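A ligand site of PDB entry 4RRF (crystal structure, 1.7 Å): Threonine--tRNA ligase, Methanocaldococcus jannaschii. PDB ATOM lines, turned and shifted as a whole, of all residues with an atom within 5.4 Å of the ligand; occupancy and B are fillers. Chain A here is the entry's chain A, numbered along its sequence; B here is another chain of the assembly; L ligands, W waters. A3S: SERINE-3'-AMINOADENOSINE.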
ATOM      1  N   THR A  19     -15.893 -12.148 -30.158  1.00  0.00           N
ATOM      2  CA  THR A  19     -17.181 -12.516 -29.564  1.00  0.00           C
ATOM      3  C   THR A  19     -17.811 -11.263 -28.935  1.00  0.00           C
ATOM      4  O   THR A  19     -17.183 -10.206 -28.810  1.00  0.00           O
ATOM      5  CB  THR A  19     -17.068 -13.589 -28.454  1.00  0.00           C
ATOM      6  OG1 THR A  19     -16.487 -13.009 -27.271  1.00  0.00           O
ATOM      7  CG2 THR A  19     -16.271 -14.833 -28.913  1.00  0.00           C
ATOM      8  N   ILE A  21     -17.892 -10.561 -25.967  1.00  0.00           N
ATOM      9  CA  ILE A  21     -17.102 -10.201 -24.764  1.00  0.00           C
ATOM     10  C   ILE A  21     -15.593  -9.980 -25.081  1.00  0.00           C
ATOM     11  O   ILE A  21     -14.741  -9.910 -24.190  1.00  0.00           O
ATOM     12  CB  ILE A  21     -17.358 -11.229 -23.611  1.00  0.00           C
ATOM     13  CG1 ILE A  21     -16.930 -12.658 -24.049  1.00  0.00           C
ATOM     14  CG2 ILE A  21     -18.819 -11.084 -23.127  1.00  0.00           C
ATOM     15  CD1 ILE A  21     -16.914 -13.778 -22.997  1.00  0.00           C
ATOM     16  N   ILE A  40      -6.344 -21.556 -18.865  1.00  0.00           N
ATOM     17  CA  ILE A  40      -7.100 -21.291 -17.616  1.00  0.00           C
ATOM     18  C   ILE A  40      -8.576 -21.024 -17.868  1.00  0.00           C
ATOM     19  O   ILE A  40      -8.923 -20.181 -18.671  1.00  0.00           O
ATOM     20  CB  ILE A  40      -6.532 -20.065 -16.861  1.00  0.00           C
ATOM     21  CG1 ILE A  40      -5.083 -20.297 -16.468  1.00  0.00           C
ATOM     22  CG2 ILE A  40      -7.389 -19.686 -15.668  1.00  0.00           C
ATOM     23  CD1 ILE A  40      -4.352 -19.032 -16.037  1.00  0.00           C
ATOM     24  N   ALA A  41      -9.429 -21.791 -17.176  1.00  0.00           N
ATOM     25  CA  ALA A  41     -10.845 -21.570 -17.192  1.00  0.00           C
ATOM     26  C   ALA A  41     -11.224 -21.038 -15.780  1.00  0.00           C
ATOM     27  O   ALA A  41     -11.000 -21.720 -14.747  1.00  0.00           O
ATOM     28  CB  ALA A  41     -11.557 -22.925 -17.516  1.00  0.00           C
ATOM     29  N   VAL A  42     -11.790 -19.833 -15.735  1.00  0.00           N
ATOM     30  CA  VAL A  42     -12.244 -19.238 -14.450  1.00  0.00           C
ATOM     31  C   VAL A  42     -13.675 -19.721 -14.188  1.00  0.00           C
ATOM     32  O   VAL A  42     -14.539 -19.591 -15.058  1.00  0.00           O
ATOM     33  CB  VAL A  42     -12.218 -17.685 -14.392  1.00  0.00           C
ATOM     34  CG1 VAL A  42     -12.369 -17.233 -12.948  1.00  0.00           C
ATOM     35  CG2 VAL A  42     -10.921 -17.072 -14.894  1.00  0.00           C
ATOM     36  N   GLU A  43     -13.907 -20.255 -13.018  1.00  0.00           N
ATOM     37  CA  GLU A  43     -15.135 -21.015 -12.744  1.00  0.00           C
ATOM     38  C   GLU A  43     -16.073 -20.257 -11.836  1.00  0.00           C
ATOM     39  O   GLU A  43     -15.679 -19.312 -11.201  1.00  0.00           O
ATOM     40  CB  GLU A  43     -14.782 -22.365 -12.123  1.00  0.00           C
ATOM     41  CG  GLU A  43     -14.042 -23.269 -13.086  1.00  0.00           C
ATOM     42  CD  GLU A  43     -13.810 -24.647 -12.524  1.00  0.00           C
ATOM     43  OE1 GLU A  43     -13.195 -24.751 -11.418  1.00  0.00           O
ATOM     44  OE2 GLU A  43     -14.195 -25.647 -13.172  1.00  0.00           O
ATOM     45  N   TYR A  76      -3.388 -17.917 -20.726  1.00  0.00           N
ATOM     46  CA  TYR A  76      -4.207 -18.133 -21.906  1.00  0.00           C
ATOM     47  C   TYR A  76      -5.610 -18.526 -21.505  1.00  0.00           C
ATOM     48  O   TYR A  76      -5.820 -19.610 -20.975  1.00  0.00           O
ATOM     49  CB  TYR A  76      -3.542 -19.214 -22.734  1.00  0.00           C
ATOM     50  CG  TYR A  76      -3.997 -19.306 -24.145  1.00  0.00           C
ATOM     51  CD1 TYR A  76      -5.201 -19.986 -24.492  1.00  0.00           C
ATOM     52  CD2 TYR A  76      -3.233 -18.729 -25.145  1.00  0.00           C
ATOM     53  CE1 TYR A  76      -5.542 -20.091 -25.826  1.00  0.00           C
ATOM     54  CE2 TYR A  76      -3.606 -18.826 -26.474  1.00  0.00           C
ATOM     55  CZ  TYR A  76      -4.768 -19.500 -26.788  1.00  0.00           C
ATOM     56  OH  TYR A  76      -5.122 -19.639 -28.114  1.00  0.00           O
ATOM     57  N   PRO A  77      -6.582 -17.613 -21.723  1.00  0.00           N
ATOM     58  CA  PRO A  77      -7.986 -17.941 -21.347  1.00  0.00           C
ATOM     59  C   PRO A  77      -8.453 -19.104 -22.146  1.00  0.00           C
ATOM     60  O   PRO A  77      -8.173 -19.150 -23.349  1.00  0.00           O
ATOM     61  CB  PRO A  77      -8.766 -16.667 -21.738  1.00  0.00           C
ATOM     62  CG  PRO A  77      -7.721 -15.578 -21.762  1.00  0.00           C
ATOM     63  CD  PRO A  77      -6.456 -16.243 -22.246  1.00  0.00           C
ATOM     64  N   TYR A  78      -9.050 -20.097 -21.468  1.00  0.00           N
ATOM     65  CA  TYR A  78      -9.393 -21.356 -22.115  1.00  0.00           C
ATOM     66  C   TYR A  78     -10.653 -21.918 -21.494  1.00  0.00           C
ATOM     67  O   TYR A  78     -10.599 -22.779 -20.604  1.00  0.00           O
ATOM     68  CB  TYR A  78      -8.233 -22.355 -22.015  1.00  0.00           C
ATOM     69  CG  TYR A  78      -8.152 -23.207 -23.258  1.00  0.00           C
ATOM     70  CD1 TYR A  78      -7.743 -22.640 -24.472  1.00  0.00           C
ATOM     71  CD2 TYR A  78      -8.529 -24.575 -23.262  1.00  0.00           C
ATOM     72  CE1 TYR A  78      -7.701 -23.393 -25.632  1.00  0.00           C
ATOM     73  CE2 TYR A  78      -8.481 -25.336 -24.444  1.00  0.00           C
ATOM     74  CZ  TYR A  78      -8.040 -24.726 -25.628  1.00  0.00           C
ATOM     75  OH  TYR A  78      -7.951 -25.419 -26.823  1.00  0.00           O
ATOM     76  N   ALA A  79     -11.768 -21.447 -21.997  1.00  0.00           N
ATOM     77  CA  ALA A  79     -12.974 -21.654 -21.221  1.00  0.00           C
ATOM     78  C   ALA A  79     -13.378 -23.111 -21.363  1.00  0.00           C
ATOM     79  O   ALA A  79     -14.132 -23.631 -20.558  1.00  0.00           O
ATOM     80  CB  ALA A  79     -14.064 -20.758 -21.791  1.00  0.00           C
ATOM     81  N   HIS A  80     -12.802 -23.801 -22.347  1.00  0.00           N
ATOM     82  CA  HIS A  80     -13.202 -25.207 -22.634  1.00  0.00           C
ATOM     83  C   HIS A  80     -12.835 -26.196 -21.546  1.00  0.00           C
ATOM     84  O   HIS A  80     -13.316 -27.337 -21.554  1.00  0.00           O
ATOM     85  CB  HIS A  80     -12.644 -25.668 -23.973  1.00  0.00           C
ATOM     86  CG  HIS A  80     -12.663 -24.601 -25.020  1.00  0.00           C
ATOM     87  ND1 HIS A  80     -13.741 -24.387 -25.811  1.00  0.00           N
ATOM     88  CD2 HIS A  80     -11.733 -23.623 -25.336  1.00  0.00           C
ATOM     89  CE1 HIS A  80     -13.483 -23.364 -26.634  1.00  0.00           C
ATOM     90  NE2 HIS A  80     -12.266 -22.882 -26.340  1.00  0.00           N
ATOM     91  N   LEU A  85     -18.674 -22.063 -15.842  1.00  0.00           N
ATOM     92  CA  LEU A  85     -17.803 -20.891 -15.904  1.00  0.00           C
ATOM     93  C   LEU A  85     -18.218 -19.730 -15.048  1.00  0.00           C
ATOM     94  O   LEU A  85     -19.423 -19.474 -14.877  1.00  0.00           O
ATOM     95  CB  LEU A  85     -17.714 -20.420 -17.370  1.00  0.00           C
ATOM     96  CG  LEU A  85     -17.034 -21.387 -18.354  1.00  0.00           C
ATOM     97  CD1 LEU A  85     -17.157 -20.797 -19.762  1.00  0.00           C
ATOM     98  CD2 LEU A  85     -15.584 -21.753 -18.019  1.00  0.00           C
ATOM     99  N   SER A  86     -17.254 -18.947 -14.559  1.00  0.00           N
ATOM    100  CA  SER A  86     -17.613 -17.655 -14.025  1.00  0.00           C
ATOM    101  C   SER A  86     -18.176 -16.674 -15.065  1.00  0.00           C
ATOM    102  O   SER A  86     -18.049 -16.841 -16.306  1.00  0.00           O
ATOM    103  CB  SER A  86     -16.412 -17.001 -13.324  1.00  0.00           C
ATOM    104  OG  SER A  86     -15.576 -16.412 -14.325  1.00  0.00           O
ATOM    105  N   SER A  87     -18.763 -15.584 -14.588  1.00  0.00           N
ATOM    106  CA  SER A  87     -19.133 -14.462 -15.468  1.00  0.00           C
ATOM    107  C   SER A  87     -17.877 -13.909 -16.210  1.00  0.00           C
ATOM    108  O   SER A  87     -16.733 -14.062 -15.749  1.00  0.00           O
ATOM    109  CB  SER A  87     -19.753 -13.355 -14.623  1.00  0.00           C
ATOM    110  OG  SER A  87     -18.710 -12.677 -13.920  1.00  0.00           O
ATOM    111  N   PRO A  88     -18.066 -13.265 -17.363  1.00  0.00           N
ATOM    112  CA  PRO A  88     -16.896 -12.676 -18.040  1.00  0.00           C
ATOM    113  C   PRO A  88     -16.217 -11.597 -17.205  1.00  0.00           C
ATOM    114  O   PRO A  88     -14.979 -11.509 -17.250  1.00  0.00           O
ATOM    115  CB  PRO A  88     -17.451 -12.137 -19.351  1.00  0.00           C
ATOM    116  CG  PRO A  88     -18.853 -12.641 -19.439  1.00  0.00           C
ATOM    117  CD  PRO A  88     -19.336 -12.971 -18.069  1.00  0.00           C
ATOM    118  N   ALA A  91     -13.991 -13.246 -14.821  1.00  0.00           N
ATOM    119  CA  ALA A  91     -12.933 -14.021 -15.481  1.00  0.00           C
ATOM    120  C   ALA A  91     -11.793 -13.100 -15.902  1.00  0.00           C
ATOM    121  O   ALA A  91     -10.631 -13.416 -15.611  1.00  0.00           O
ATOM    122  CB  ALA A  91     -13.483 -14.791 -16.679  1.00  0.00           C
ATOM    123  N   LEU A  95      -7.885 -13.231 -14.507  1.00  0.00           N
ATOM    124  CA  LEU A  95      -6.757 -13.431 -15.490  1.00  0.00           C
ATOM    125  C   LEU A  95      -5.772 -12.252 -15.375  1.00  0.00           C
ATOM    126  O   LEU A  95      -4.545 -12.475 -15.393  1.00  0.00           O
ATOM    127  CB  LEU A  95      -7.330 -13.495 -16.910  1.00  0.00           C
ATOM    128  CG  LEU A  95      -8.149 -14.803 -17.044  1.00  0.00           C
ATOM    129  CD1 LEU A  95      -9.041 -14.787 -18.262  1.00  0.00           C
ATOM    130  CD2 LEU A  95      -7.181 -15.976 -17.124  1.00  0.00           C
ATOM    131  N   PRO A 113      -5.527 -12.325 -25.253  1.00  0.00           N
ATOM    132  CA  PRO A 113      -6.668 -11.440 -25.017  1.00  0.00           C
ATOM    133  C   PRO A 113      -7.934 -12.265 -24.716  1.00  0.00           C
ATOM    134  O   PRO A 113      -8.093 -13.394 -25.220  1.00  0.00           O
ATOM    135  CB  PRO A 113      -6.812 -10.677 -26.360  1.00  0.00           C
ATOM    136  CG  PRO A 113      -6.247 -11.597 -27.348  1.00  0.00           C
ATOM    137  CD  PRO A 113      -5.038 -12.202 -26.647  1.00  0.00           C
ATOM    138  N   PHE A 114      -8.751 -11.729 -23.843  1.00  0.00           N
ATOM    139  CA  PHE A 114      -9.964 -12.397 -23.357  1.00  0.00           C
ATOM    140  C   PHE A 114     -11.073 -12.214 -24.377  1.00  0.00           C
ATOM    141  O   PHE A 114     -11.240 -11.131 -24.954  1.00  0.00           O
ATOM    142  CB  PHE A 114     -10.408 -11.756 -22.047  1.00  0.00           C
ATOM    143  CG  PHE A 114     -11.581 -12.401 -21.418  1.00  0.00           C
ATOM    144  CD1 PHE A 114     -11.424 -13.524 -20.620  1.00  0.00           C
ATOM    145  CD2 PHE A 114     -12.863 -11.895 -21.663  1.00  0.00           C
ATOM    146  CE1 PHE A 114     -12.544 -14.119 -20.071  1.00  0.00           C
ATOM    147  CE2 PHE A 114     -13.992 -12.518 -21.124  1.00  0.00           C
ATOM    148  CZ  PHE A 114     -13.810 -13.641 -20.310  1.00  0.00           C
ATOM    149  N   GLY A 115     -11.829 -13.261 -24.604  1.00  0.00           N
ATOM    150  CA  GLY A 115     -13.102 -13.103 -25.328  1.00  0.00           C
ATOM    151  C   GLY A 115     -12.982 -13.203 -26.850  1.00  0.00           C
ATOM    152  O   GLY A 115     -13.861 -12.726 -27.552  1.00  0.00           O
ATOM    153  N   TRP A 116     -11.874 -13.775 -27.336  1.00  0.00           N
ATOM    154  CA  TRP A 116     -11.695 -14.010 -28.776  1.00  0.00           C
ATOM    155  C   TRP A 116     -11.601 -15.462 -29.108  1.00  0.00           C
ATOM    156  O   TRP A 116     -11.154 -16.287 -28.275  1.00  0.00           O
ATOM    157  CB  TRP A 116     -10.401 -13.400 -29.269  1.00  0.00           C
ATOM    158  CG  TRP A 116     -10.322 -11.912 -29.270  1.00  0.00           C
ATOM    159  CD1 TRP A 116     -10.118 -11.037 -28.199  1.00  0.00           C
ATOM    160  CD2 TRP A 116     -10.420 -11.051 -30.436  1.00  0.00           C
ATOM    161  NE1 TRP A 116     -10.107  -9.749 -28.612  1.00  0.00           N
ATOM    162  CE2 TRP A 116     -10.293  -9.685 -29.959  1.00  0.00           C
ATOM    163  CE3 TRP A 116     -10.599 -11.275 -31.808  1.00  0.00           C
ATOM    164  CZ2 TRP A 116     -10.277  -8.600 -30.811  1.00  0.00           C
ATOM    165  CZ3 TRP A 116     -10.604 -10.185 -32.664  1.00  0.00           C
ATOM    166  CH2 TRP A 116     -10.448  -8.878 -32.165  1.00  0.00           C
ATOM    167  N   TYR A 117     -11.923 -15.820 -30.360  1.00  0.00           N
ATOM    168  CA  TYR A 117     -11.583 -17.120 -30.846  1.00  0.00           C
ATOM    169  C   TYR A 117     -10.209 -16.968 -31.428  1.00  0.00           C
ATOM    170  O   TYR A 117      -9.956 -16.048 -32.196  1.00  0.00           O
ATOM    171  CB  TYR A 117     -12.641 -17.612 -31.873  1.00  0.00           C
ATOM    172  CG  TYR A 117     -13.873 -18.134 -31.181  1.00  0.00           C
ATOM    173  CD1 TYR A 117     -13.795 -19.314 -30.450  1.00  0.00           C
ATOM    174  CD2 TYR A 117     -15.132 -17.480 -31.294  1.00  0.00           C
ATOM    175  CE1 TYR A 117     -14.891 -19.824 -29.775  1.00  0.00           C
ATOM    176  CE2 TYR A 117     -16.235 -18.000 -30.645  1.00  0.00           C
ATOM    177  CZ  TYR A 117     -16.102 -19.172 -29.878  1.00  0.00           C
ATOM    178  OH  TYR A 117     -17.178 -19.772 -29.213  1.00  0.00           O
ATOM    179  N   LYS A 118      -9.277 -17.845 -31.018  1.00  0.00           N
ATOM    180  CA  LYS A 118      -7.921 -17.663 -31.435  1.00  0.00           C
ATOM    181  C   LYS A 118      -7.255 -18.882 -31.993  1.00  0.00           C
ATOM    182  O   LYS A 118      -7.504 -20.021 -31.541  1.00  0.00           O
ATOM    183  CB  LYS A 118      -7.036 -17.211 -30.237  1.00  0.00           C
ATOM    184  CG  LYS A 118      -7.594 -15.993 -29.505  1.00  0.00           C
ATOM    185  CD  LYS A 118      -6.591 -15.393 -28.536  1.00  0.00           C
ATOM    186  CE  LYS A 118      -6.471 -16.257 -27.313  1.00  0.00           C
ATOM    187  NZ  LYS A 118      -7.794 -16.456 -26.711  1.00  0.00           N
ATOM    188  N   GLY B 126      -8.503 -21.774 -35.037  1.00  0.00           N
ATOM    189  CA  GLY B 126      -8.898 -20.542 -34.369  1.00  0.00           C
ATOM    190  C   GLY B 126     -10.291 -19.951 -34.648  1.00  0.00           C
ATOM    191  O   GLY B 126     -10.517 -18.775 -34.457  1.00  0.00           O
ATOM    192  N   SER B 130     -13.616 -24.292 -33.529  1.00  0.00           N
ATOM    193  CA  SER B 130     -12.284 -24.941 -33.632  1.00  0.00           C
ATOM    194  C   SER B 130     -11.870 -25.647 -32.337  1.00  0.00           C
ATOM    195  O   SER B 130     -10.907 -26.429 -32.329  1.00  0.00           O
ATOM    196  CB  SER B 130     -11.222 -23.977 -34.165  1.00  0.00           C
ATOM    197  OG  SER B 130     -10.846 -22.978 -33.211  1.00  0.00           O
ATOM    198  N   GLU B 131     -12.586 -25.384 -31.239  1.00  0.00           N
ATOM    199  CA  GLU B 131     -12.291 -26.033 -29.957  1.00  0.00           C
ATOM    200  C   GLU B 131     -13.663 -26.247 -29.328  1.00  0.00           C
ATOM    201  O   GLU B 131     -14.442 -25.285 -29.157  1.00  0.00           O
ATOM    202  CB  GLU B 131     -11.419 -25.161 -29.017  1.00  0.00           C
ATOM    203  CG  GLU B 131     -10.068 -24.742 -29.592  1.00  0.00           C
ATOM    204  CD  GLU B 131      -9.420 -23.623 -28.764  1.00  0.00           C
ATOM    205  OE1 GLU B 131      -8.250 -23.317 -28.999  1.00  0.00           O
ATOM    206  OE2 GLU B 131     -10.072 -23.083 -27.850  1.00  0.00           O
HETATM  207  O5' A3S L   1     -15.916 -17.949 -24.411  1.00  0.00           O
HETATM  208  C5' A3S L   1     -15.365 -17.192 -25.485  1.00  0.00           C
HETATM  209  C4' A3S L   1     -14.037 -16.644 -25.082  1.00  0.00           C
HETATM  210  O4' A3S L   1     -14.345 -15.961 -23.941  1.00  0.00           O
HETATM  211  C1' A3S L   1     -13.312 -16.261 -22.951  1.00  0.00           C
HETATM  212  N9  A3S L   1     -13.957 -16.792 -21.718  1.00  0.00           N
HETATM  213  C4  A3S L   1     -13.347 -17.315 -20.678  1.00  0.00           C
HETATM  214  N3  A3S L   1     -12.079 -17.773 -20.454  1.00  0.00           N
HETATM  215  C2  A3S L   1     -11.754 -18.303 -19.248  1.00  0.00           C
HETATM  216  N1  A3S L   1     -12.633 -18.469 -18.256  1.00  0.00           N
HETATM  217  C6  A3S L   1     -13.916 -18.013 -18.451  1.00  0.00           C
HETATM  218  N6  A3S L   1     -14.798 -18.152 -17.452  1.00  0.00           N
HETATM  219  C5  A3S L   1     -14.302 -17.466 -19.678  1.00  0.00           C
HETATM  220  N7  A3S L   1     -15.500 -16.906 -20.154  1.00  0.00           N
HETATM  221  C8  A3S L   1     -15.264 -16.467 -21.413  1.00  0.00           C
HETATM  222  C2' A3S L   1     -12.213 -17.015 -23.606  1.00  0.00           C
HETATM  223  O2' A3S L   1     -11.314 -16.052 -24.189  1.00  0.00           O
HETATM  224  C3' A3S L   1     -13.080 -17.784 -24.634  1.00  0.00           C
HETATM  225  N8  A3S L   1     -12.230 -18.169 -25.745  1.00  0.00           N
HETATM  226  N   A3S L   1      -9.566 -20.604 -26.556  1.00  0.00           N
HETATM  227  CA  A3S L   1     -10.467 -19.469 -26.855  1.00  0.00           C
HETATM  228  CB  A3S L   1     -11.199 -19.805 -28.176  1.00  0.00           C
HETATM  229  OG  A3S L   1     -10.180 -19.801 -29.191  1.00  0.00           O
HETATM  230  C   A3S L   1     -11.454 -19.244 -25.693  1.00  0.00           C
HETATM  231  O   A3S L   1     -11.413 -20.067 -24.604  1.00  0.00           O
HETATM  232  O   HOH W   1     -18.413 -17.244 -23.066  1.00  0.00           O
HETATM  233  O   HOH W   2      -7.536 -20.790 -28.675  1.00  0.00           O
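The side-chain hydroxyl (OG1) of Thr 19 sits at hydrogen-bond distance from the backbone carbonyl oxygen (O) of Gly 115. NZ of Lys 118 sits at hydrogen-bond distance from O of Pro 113 (3.4 Å). OG1 of Thr 19 lies close to N of Ile 21. The side-chain hydroxyl (OH) of Tyr 78 lies close to the side-chain carboxylate (OE1) of Glu 131 of chain B. A ring nitrogen (NE2) of His 80 sits at hydrogen-bond distance from the side-chain carboxylate of Glu 131 of chain B, 2.7 Å away. The backbone carbonyl oxygen (O) of Val 42 lies within hydrogen-bond range of the backbone NH (N) of Ser 86 (2.8 Å). The backbone carbonyl oxygen (O) of Tyr 76 sits at hydrogen-bond distance from the backbone NH (N) of Ile 40, at 2.9 Å. O of Ile 40 lies within hydrogen-bond range of N of Tyr 78 (2.8 Å).
N of Ala 79 is in hydrogen-bond range of O of the ligand (3.0 Å). O of Val 42 lies within hydrogen-bond range of N6 of the ligand (2.8 Å). The backbone NH of Val 42 is in hydrogen-bond range of a nitrogen (N1) of the ligand, at 3.0 Å. An oxygen (O) of the ligand sits at hydrogen-bond distance from a ring nitrogen (NE2) of His 80 (3.4 Å). N of the ligand is in salt-bridge range of OE2 of Glu 131 of chain B (2.8 Å). A nitrogen (N8) of the ligand is in hydrogen-bond range of the backbone carbonyl oxygen of Trp 116, at 3.3 Å. N of Lys 118 is in hydrogen-bond range of OG of the ligand (2.8 Å). The backbone NH (N) of Gly 115 sits at hydrogen-bond distance from an oxygen (O2') of the ligand (2.9 Å).
Ile 21 touches the ligand. Ile 40 touches the ligand. CA of Ala 41 touches N1 of the ligand, at 3.7 Å. Pro 77 touches the ligand. Tyr 78 touches the ligand (CD1 to N, 3.4 Å). CB of Leu 85 touches N6 of the ligand, 3.7 Å away. Ser 86 touches the ligand. Ala 91 touches the ligand (CB to N6, 3.7 Å). Phe 114 touches the ligand. Tyr 117 touches the ligand. Hydrophobic or aromatic side chains within 4 Å of the ligand: Ile 21, Val 42, Pro 77, Tyr 78, Ala 79, His 80, Leu 85, Ala 91, Phe 114 and Tyr 117. 17 residues have an atom within 4 Å of the ligand: Ile 21, Ile 40, Ala 41, Val 42, Pro 77, Tyr 78, Ala 79, His 80, Leu 85, Ser 86, Ala 91, Phe 114, Gly 115, Trp 116, Tyr 117, Lys 118 and Glu 131 of chain B. Along chain A the residues within 4 Å of the ligand span positions 21 to 118.
Water W2 lies within hydrogen-bond range of the side-chain carboxylate of Glu 131 of chain B (2.6 Å), the side-chain hydroxyl of Tyr 76 (2.7 Å), an oxygen (OG) of the ligand (2.9 Å) and the backbone carbonyl oxygen of Lys 118 (3.0 Å).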
